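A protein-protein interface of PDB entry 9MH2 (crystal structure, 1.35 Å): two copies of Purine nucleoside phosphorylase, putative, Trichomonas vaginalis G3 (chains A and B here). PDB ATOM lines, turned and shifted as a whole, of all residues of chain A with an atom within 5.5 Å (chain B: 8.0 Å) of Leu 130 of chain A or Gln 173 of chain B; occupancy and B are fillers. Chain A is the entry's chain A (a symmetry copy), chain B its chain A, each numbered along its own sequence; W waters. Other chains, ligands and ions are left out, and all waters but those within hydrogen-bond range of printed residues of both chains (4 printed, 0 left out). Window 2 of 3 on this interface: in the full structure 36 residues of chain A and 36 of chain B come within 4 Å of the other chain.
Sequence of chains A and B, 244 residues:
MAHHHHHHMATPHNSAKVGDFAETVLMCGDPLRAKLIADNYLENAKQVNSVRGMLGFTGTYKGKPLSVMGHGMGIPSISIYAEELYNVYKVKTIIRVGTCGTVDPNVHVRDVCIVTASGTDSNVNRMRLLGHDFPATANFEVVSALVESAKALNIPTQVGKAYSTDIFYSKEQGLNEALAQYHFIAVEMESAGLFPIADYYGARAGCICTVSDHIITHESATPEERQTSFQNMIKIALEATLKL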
ATOM      1  N   ARG A 126      22.720 -22.170  18.129  1.00  0.00           N
ATOM      2  CA  ARG A 126      23.583 -21.277  18.899  1.00  0.00           C
ATOM      3  C   ARG A 126      22.758 -20.415  19.845  1.00  0.00           C
ATOM      4  O   ARG A 126      23.163 -20.173  20.984  1.00  0.00           O
ATOM      5  CB  ARG A 126      24.403 -20.421  17.940  1.00  0.00           C
ATOM      6  CG  ARG A 126      25.375 -21.253  17.138  1.00  0.00           C
ATOM      7  CD  ARG A 126      26.189 -20.421  16.160  1.00  0.00           C
ATOM      8  NE  ARG A 126      26.971 -21.344  15.350  1.00  0.00           N
ATOM      9  CZ  ARG A 126      27.863 -21.002  14.434  1.00  0.00           C
ATOM     10  NH1 ARG A 126      28.113 -19.739  14.151  1.00  0.00           N
ATOM     11  NH2 ARG A 126      28.535 -21.961  13.799  1.00  0.00           N
ATOM     12  N   MET A 127      21.588 -19.944  19.393  1.00  0.00           N
ATOM     13  CA  MET A 127      20.784 -19.098  20.265  1.00  0.00           C
ATOM     14  C   MET A 127      20.237 -19.846  21.468  1.00  0.00           C
ATOM     15  O   MET A 127      19.902 -19.209  22.470  1.00  0.00           O
ATOM     16  CB  MET A 127      19.673 -18.437  19.464  1.00  0.00           C
ATOM     17  CG  MET A 127      20.242 -17.465  18.454  1.00  0.00           C
ATOM     18  SD  MET A 127      19.041 -16.426  17.628  1.00  0.00           S
ATOM     19  CE  MET A 127      18.225 -17.589  16.533  1.00  0.00           C
ATOM     20  N   ARG A 128      20.173 -21.179  21.412  1.00  0.00           N
ATOM     21  CA  ARG A 128      19.699 -21.979  22.526  1.00  0.00           C
ATOM     22  C   ARG A 128      20.787 -22.319  23.533  1.00  0.00           C
ATOM     23  O   ARG A 128      20.460 -22.676  24.670  1.00  0.00           O
ATOM     24  CB  ARG A 128      19.115 -23.297  22.012  1.00  0.00           C
ATOM     25  CG  ARG A 128      17.880 -23.123  21.157  1.00  0.00           C
ATOM     26  CD  ARG A 128      17.366 -24.453  20.572  1.00  0.00           C
ATOM     27  NE  ARG A 128      15.972 -24.348  20.125  1.00  0.00           N
ATOM     28  CZ  ARG A 128      15.559 -24.298  18.864  1.00  0.00           C
ATOM     29  NH1 ARG A 128      16.390 -24.486  17.849  1.00  0.00           N
ATOM     30  NH2 ARG A 128      14.272 -24.061  18.611  1.00  0.00           N
ATOM     31  N   LEU A 129      22.066 -22.228  23.161  1.00  0.00           N
ATOM     32  CA  LEU A 129      23.151 -22.709  24.016  1.00  0.00           C
ATOM     33  C   LEU A 129      24.245 -21.665  24.141  1.00  0.00           C
ATOM     34  O   LEU A 129      25.436 -21.954  24.028  1.00  0.00           O
ATOM     35  CB  LEU A 129      23.681 -24.050  23.518  1.00  0.00           C
ATOM     36  CG  LEU A 129      24.390 -24.902  24.572  1.00  0.00           C
ATOM     37  CD1 LEU A 129      23.404 -25.306  25.661  1.00  0.00           C
ATOM     38  CD2 LEU A 129      25.003 -26.146  23.930  1.00  0.00           C
ATOM     39  N   LEU A 130      23.843 -20.424  24.394  1.00  0.00           N
ATOM     40  CA  LEU A 130      24.776 -19.363  24.779  1.00  0.00           C
ATOM     41  C   LEU A 130      25.834 -19.123  23.705  1.00  0.00           C
ATOM     42  O   LEU A 130      26.964 -18.728  24.002  1.00  0.00           O
ATOM     43  CB  LEU A 130      25.418 -19.649  26.146  1.00  0.00           C
ATOM     44  CG  LEU A 130      24.528 -19.398  27.367  1.00  0.00           C
ATOM     45  CD1 LEU A 130      23.351 -20.330  27.402  1.00  0.00           C
ATOM     46  CD2 LEU A 130      25.310 -19.501  28.668  1.00  0.00           C
ATOM     47  N   GLY A 131      25.480 -19.373  22.450  1.00  0.00           N
ATOM     48  CA  GLY A 131      26.358 -19.142  21.330  1.00  0.00           C
ATOM     49  C   GLY A 131      27.250 -20.298  20.961  1.00  0.00           C
ATOM     50  O   GLY A 131      27.987 -20.194  19.978  1.00  0.00           O
ATOM     51  N   HIS A 132      27.178 -21.406  21.685  1.00  0.00           N
ATOM     52  CA  HIS A 132      28.102 -22.516  21.509  1.00  0.00           C
ATOM     53  C   HIS A 132      27.548 -23.516  20.497  1.00  0.00           C
ATOM     54  O   HIS A 132      26.508 -23.283  19.872  1.00  0.00           O
ATOM     55  CB  HIS A 132      28.383 -23.167  22.855  1.00  0.00           C
ATOM     56  CG  HIS A 132      28.866 -22.208  23.887  1.00  0.00           C
ATOM     57  ND1 HIS A 132      29.936 -21.365  23.674  1.00  0.00           N
ATOM     58  CD2 HIS A 132      28.429 -21.956  25.143  1.00  0.00           C
ATOM     59  CE1 HIS A 132      30.138 -20.637  24.758  1.00  0.00           C
ATOM     60  NE2 HIS A 132      29.239 -20.981  25.665  1.00  0.00           N
ATOM     61  N   ASP B 121      32.155 -25.720  23.431  1.00  0.00           N
ATOM     62  CA  ASP B 121      32.469 -24.302  23.331  1.00  0.00           C
ATOM     63  C   ASP B 121      33.776 -24.054  22.583  1.00  0.00           C
ATOM     64  O   ASP B 121      34.223 -22.905  22.489  1.00  0.00           O
ATOM     65  CB  ASP B 121      32.469 -23.648  24.716  1.00  0.00           C
ATOM     66  CG  ASP B 121      33.349 -24.366  25.718  1.00  0.00           C
ATOM     67  OD1 ASP B 121      34.229 -25.148  25.302  1.00  0.00           O
ATOM     68  OD2 ASP B 121      33.142 -24.160  26.939  1.00  0.00           O
ATOM     69  N   ARG B 126      33.790 -25.777  13.997  1.00  0.00           N
ATOM     70  CA  ARG B 126      33.510 -24.691  13.061  1.00  0.00           C
ATOM     71  C   ARG B 126      34.626 -24.567  12.031  1.00  0.00           C
ATOM     72  O   ARG B 126      34.364 -24.324  10.852  1.00  0.00           O
ATOM     73  CB  ARG B 126      33.325 -23.393  13.838  1.00  0.00           C
ATOM     74  CG  ARG B 126      32.095 -23.435  14.714  1.00  0.00           C
ATOM     75  CD  ARG B 126      31.902 -22.158  15.515  1.00  0.00           C
ATOM     76  NE  ARG B 126      30.784 -22.377  16.420  1.00  0.00           N
ATOM     77  CZ  ARG B 126      30.259 -21.473  17.232  1.00  0.00           C
ATOM     78  NH1 ARG B 126      30.741 -20.248  17.306  1.00  0.00           N
ATOM     79  NH2 ARG B 126      29.206 -21.807  17.975  1.00  0.00           N
ATOM     80  N   TYR B 163      28.444 -32.615  26.571  1.00  0.00           N
ATOM     81  CA  TYR B 163      28.966 -31.283  26.293  1.00  0.00           C
ATOM     82  C   TYR B 163      30.437 -31.301  26.675  1.00  0.00           C
ATOM     83  O   TYR B 163      30.771 -31.553  27.836  1.00  0.00           O
ATOM     84  CB  TYR B 163      28.213 -30.232  27.100  1.00  0.00           C
ATOM     85  CG  TYR B 163      28.573 -28.803  26.764  1.00  0.00           C
ATOM     86  CD1 TYR B 163      28.144 -28.222  25.581  1.00  0.00           C
ATOM     87  CD2 TYR B 163      29.323 -28.024  27.627  1.00  0.00           C
ATOM     88  CE1 TYR B 163      28.448 -26.929  25.268  1.00  0.00           C
ATOM     89  CE2 TYR B 163      29.635 -26.692  27.320  1.00  0.00           C
ATOM     90  CZ  TYR B 163      29.183 -26.160  26.125  1.00  0.00           C
ATOM     91  OH  TYR B 163      29.442 -24.862  25.749  1.00  0.00           O
ATOM     92  N   SER B 170      34.422 -23.373  35.125  1.00  0.00           N
ATOM     93  CA  SER B 170      33.490 -22.485  34.450  1.00  0.00           C
ATOM     94  C   SER B 170      33.114 -21.296  35.327  1.00  0.00           C
ATOM     95  O   SER B 170      32.896 -21.422  36.534  1.00  0.00           O
ATOM     96  CB  SER B 170      32.226 -23.244  34.059  1.00  0.00           C
ATOM     97  OG  SER B 170      31.276 -22.346  33.501  1.00  0.00           O
ATOM     98  N   LYS B 171      33.011 -20.132  34.695  1.00  0.00           N
ATOM     99  CA  LYS B 171      32.475 -18.936  35.330  1.00  0.00           C
ATOM    100  C   LYS B 171      31.272 -18.420  34.558  1.00  0.00           C
ATOM    101  O   LYS B 171      30.922 -17.243  34.652  1.00  0.00           O
ATOM    102  CB  LYS B 171      33.564 -17.868  35.429  1.00  0.00           C
ATOM    103  CG  LYS B 171      34.768 -18.283  36.282  1.00  0.00           C
ATOM    104  CD  LYS B 171      35.989 -17.395  36.032  1.00  0.00           C
ATOM    105  CE  LYS B 171      37.173 -17.810  36.908  1.00  0.00           C
ATOM    106  NZ  LYS B 171      37.631 -19.202  36.640  1.00  0.00           N
ATOM    107  N   GLU B 172      30.621 -19.288  33.801  1.00  0.00           N
ATOM    108  CA  GLU B 172      29.667 -18.868  32.775  1.00  0.00           C
ATOM    109  C   GLU B 172      28.234 -18.940  33.289  1.00  0.00           C
ATOM    110  O   GLU B 172      27.642 -20.022  33.381  1.00  0.00           O
ATOM    111  CB  GLU B 172      29.867 -19.725  31.527  1.00  0.00           C
ATOM    112  CG  GLU B 172      29.046 -19.301  30.358  1.00  0.00           C
ATOM    113  CD  GLU B 172      29.318 -20.121  29.120  1.00  0.00           C
ATOM    114  OE1 GLU B 172      30.057 -21.142  29.206  1.00  0.00           O
ATOM    115  OE2 GLU B 172      28.753 -19.753  28.070  1.00  0.00           O
ATOM    116  N   GLN B 173      27.653 -17.777  33.558  1.00  0.00           N
ATOM    117  CA  GLN B 173      26.274 -17.697  34.010  1.00  0.00           C
ATOM    118  C   GLN B 173      25.333 -18.277  32.964  1.00  0.00           C
ATOM    119  O   GLN B 173      25.433 -17.963  31.775  1.00  0.00           O
ATOM    120  CB  GLN B 173      25.902 -16.232  34.221  1.00  0.00           C
ATOM    121  CG  GLN B 173      26.823 -15.462  35.142  1.00  0.00           C
ATOM    122  CD  GLN B 173      26.612 -15.810  36.597  1.00  0.00           C
ATOM    123  OE1 GLN B 173      26.830 -16.947  37.013  1.00  0.00           O
ATOM    124  NE2 GLN B 173      26.184 -14.827  37.383  1.00  0.00           N
ATOM    125  N   GLY B 174      24.415 -19.121  33.409  1.00  0.00           N
ATOM    126  CA  GLY B 174      23.374 -19.628  32.549  1.00  0.00           C
ATOM    127  C   GLY B 174      23.719 -20.888  31.786  1.00  0.00           C
ATOM    128  O   GLY B 174      22.822 -21.496  31.194  1.00  0.00           O
ATOM    129  N   LEU B 175      24.983 -21.318  31.795  1.00  0.00           N
ATOM    130  CA  LEU B 175      25.359 -22.513  31.039  1.00  0.00           C
ATOM    131  C   LEU B 175      24.664 -23.758  31.584  1.00  0.00           C
ATOM    132  O   LEU B 175      24.071 -24.538  30.826  1.00  0.00           O
ATOM    133  CB  LEU B 175      26.882 -22.691  31.049  1.00  0.00           C
ATOM    134  CG  LEU B 175      27.378 -23.974  30.356  1.00  0.00           C
ATOM    135  CD1 LEU B 175      27.087 -23.953  28.861  1.00  0.00           C
ATOM    136  CD2 LEU B 175      28.877 -24.214  30.634  1.00  0.00           C
ATOM    137  N   ASN B 176      24.724 -23.967  32.901  1.00  0.00           N
ATOM    138  CA  ASN B 176      24.159 -25.190  33.464  1.00  0.00           C
ATOM    139  C   ASN B 176      22.659 -25.252  33.234  1.00  0.00           C
ATOM    140  O   ASN B 176      22.106 -26.325  32.978  1.00  0.00           O
ATOM    141  CB  ASN B 176      24.451 -25.267  34.957  1.00  0.00           C
ATOM    142  CG  ASN B 176      25.907 -25.508  35.247  1.00  0.00           C
ATOM    143  OD1 ASN B 176      26.639 -26.054  34.423  1.00  0.00           O
ATOM    144  ND2 ASN B 176      26.337 -25.093  36.417  1.00  0.00           N
ATOM    145  N   GLU B 177      21.987 -24.105  33.317  1.00  0.00           N
ATOM    146  CA  GLU B 177      20.544 -24.066  33.096  1.00  0.00           C
ATOM    147  C   GLU B 177      20.194 -24.446  31.664  1.00  0.00           C
ATOM    148  O   GLU B 177      19.221 -25.173  31.427  1.00  0.00           O
ATOM    149  CB  GLU B 177      20.025 -22.663  33.417  1.00  0.00           C
ATOM    150  CG  GLU B 177      20.003 -22.317  34.905  1.00  0.00           C
ATOM    151  CD  GLU B 177      21.367 -21.903  35.496  1.00  0.00           C
ATOM    152  OE1 GLU B 177      22.367 -21.722  34.756  1.00  0.00           O
ATOM    153  OE2 GLU B 177      21.435 -21.759  36.737  1.00  0.00           O
ATOM    154  N   ALA B 178      20.977 -23.973  30.695  1.00  0.00           N
ATOM    155  CA  ALA B 178      20.722 -24.330  29.302  1.00  0.00           C
ATOM    156  C   ALA B 178      21.024 -25.800  29.045  1.00  0.00           C
ATOM    157  O   ALA B 178      20.256 -26.491  28.368  1.00  0.00           O
ATOM    158  CB  ALA B 178      21.548 -23.442  28.372  1.00  0.00           C
ATOM    159  N   LEU B 179      22.140 -26.299  29.582  1.00  0.00           N
ATOM    160  CA  LEU B 179      22.442 -27.718  29.414  1.00  0.00           C
ATOM    161  C   LEU B 179      21.326 -28.591  29.974  1.00  0.00           C
ATOM    162  O   LEU B 179      20.950 -29.592  29.360  1.00  0.00           O
ATOM    163  CB  LEU B 179      23.777 -28.033  30.086  1.00  0.00           C
ATOM    164  CG  LEU B 179      25.014 -27.401  29.451  1.00  0.00           C
ATOM    165  CD1 LEU B 179      26.238 -27.657  30.310  1.00  0.00           C
ATOM    166  CD2 LEU B 179      25.233 -27.944  28.040  1.00  0.00           C
ATOM    167  N   TYR B 182      17.963 -28.665  27.805  1.00  0.00           N
ATOM    168  CA  TYR B 182      18.002 -29.491  26.609  1.00  0.00           C
ATOM    169  C   TYR B 182      18.489 -30.903  26.889  1.00  0.00           C
ATOM    170  O   TYR B 182      18.762 -31.657  25.951  1.00  0.00           O
ATOM    171  CB  TYR B 182      18.805 -28.795  25.517  1.00  0.00           C
ATOM    172  CG  TYR B 182      18.086 -27.535  25.066  1.00  0.00           C
ATOM    173  CD1 TYR B 182      17.098 -27.593  24.093  1.00  0.00           C
ATOM    174  CD2 TYR B 182      18.350 -26.299  25.654  1.00  0.00           C
ATOM    175  CE1 TYR B 182      16.422 -26.459  23.693  1.00  0.00           C
ATOM    176  CE2 TYR B 182      17.681 -25.149  25.250  1.00  0.00           C
ATOM    177  CZ  TYR B 182      16.707 -25.247  24.269  1.00  0.00           C
ATOM    178  OH  TYR B 182      16.014 -24.140  23.844  1.00  0.00           O
HETATM  179  O   HOH W   1      30.899 -18.654  20.254  1.00  0.00           O
HETATM  180  O   HOH W   2      13.986 -23.998  21.883  1.00  0.00           O
HETATM  181  O   HOH W   3      30.664 -23.406  27.699  1.00  0.00           O
HETATM  182  O   HOH W   4      28.768 -18.138  18.605  1.00  0.00           O
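The guanidinium group (NH2) of Arg 126 of chain B sits at hydrogen-bond distance from the backbone carbonyl oxygen (O) of Gly 131 of chain A (2.8 Å). A ring nitrogen (NE2) of His 132 of chain A sits at hydrogen-bond distance from the side-chain carboxylate (OE2) of Glu 172 of chain B (2.7 Å). NE of Arg 126 of chain A lies close to NH2 of Arg 126 of chain B (3.5 Å).
The backbone NH (N) of Glu 172 of chain B lies within hydrogen-bond range of the side-chain hydroxyl (OG) of Ser 170 of chain B. The backbone NH (N) of Gly 131 of chain A sits at hydrogen-bond distance from the backbone carbonyl oxygen (O) of Arg 126 of chain A, 2.9 Å away.
Arg 128 of chain A touches Ala 178 of chain B (O to CB, 3.9 Å). Arg 128 of chain A touches Tyr 182 of chain B (CG to OH, 3.4 Å). Leu 179 of chain B touches Leu 129 of chain A. Leu 130 of chain A touches Glu 172 of chain B (CD2 to OE2, 3.5 Å). Leu 130 of chain A touches Gly 174 of chain B. Leu 130 of chain A touches Leu 175 of chain B. Leu 130 of chain A touches Ala 178 of chain B (CD1 to CB, 3.7 Å). Asp 121 of chain B touches His 132 of chain A. His 132 of chain A touches Arg 126 of chain B (C to NH2, 3.5 Å). His 132 of chain A touches Tyr 163 of chain B (CD2 to OH, 3.1 Å).
Printed residues of chain B within 4 Å of Leu 129 of chain A: Tyr 163, Ala 178 and Leu 179. Leu 130 of chain A touches just these residues of chain B: Glu 172, Gln 173, Gly 174, Leu 175 and Ala 178. Printed residues of chain A within 4 Å of Arg 126 of chain B: Arg 126, Gly 131 and His 132. Printed residues of chain A within 4 Å of Tyr 163 of chain B: Leu 129 and His 132. Gln 173 of chain B touches one residue of chain A. Printed residues of chain A within 4 Å of Leu 175 of chain B: Leu 130. The nearest printed residue of chain A that does not touch Gln 173 of chain B is His 132 of chain A (7.8 Å). The nearest printed residue of chain B that does not touch Leu 129 of chain A is Leu 175 of chain B (5.1 Å).
Of the 7 printed residues of chain A, 6 touch a printed residue of chain B. Hydrophobic or aromatic side chains of chain A that line the printed part of chain B: Leu 129, Leu 130 and His 132. Hydrophobic or aromatic side chains of chain B that line the printed part of chain A: Tyr 163, Ala 178, Leu 179 and Tyr 182. Among the printed residues, no Asp or Glu carboxylate lies within 4 Å of a Lys or Arg side-chain nitrogen of the other chain.
Arg 126 of chain B touches its own counterpart, Arg 126 of chain A. Of the 16 pairs that touch across the chains among the printed residues, 1 has its exchanged pair printed and touching as well.
Water W4 bridges the backbone carbonyl oxygen of Gly 131 of chain A and the guanidinium group of Arg 126 of chain B. Water W2 lies within hydrogen-bond range of NE of Arg 128 of chain A (2.7 Å) and OH of Tyr 182 of chain B (2.8 Å). Water W3 lies within hydrogen-bond range of the side-chain carboxylate of Asp 121 of chain B, the side-chain hydroxyl of Tyr 163 of chain B, the side-chain carboxylate of Glu 172 of chain B and a ring nitrogen (NE2) of His 132 of chain A. Water W1 bridges O of Gly 131 of chain A (3.3 Å) and NH1 of Arg 126 of chain B (3.4 Å).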
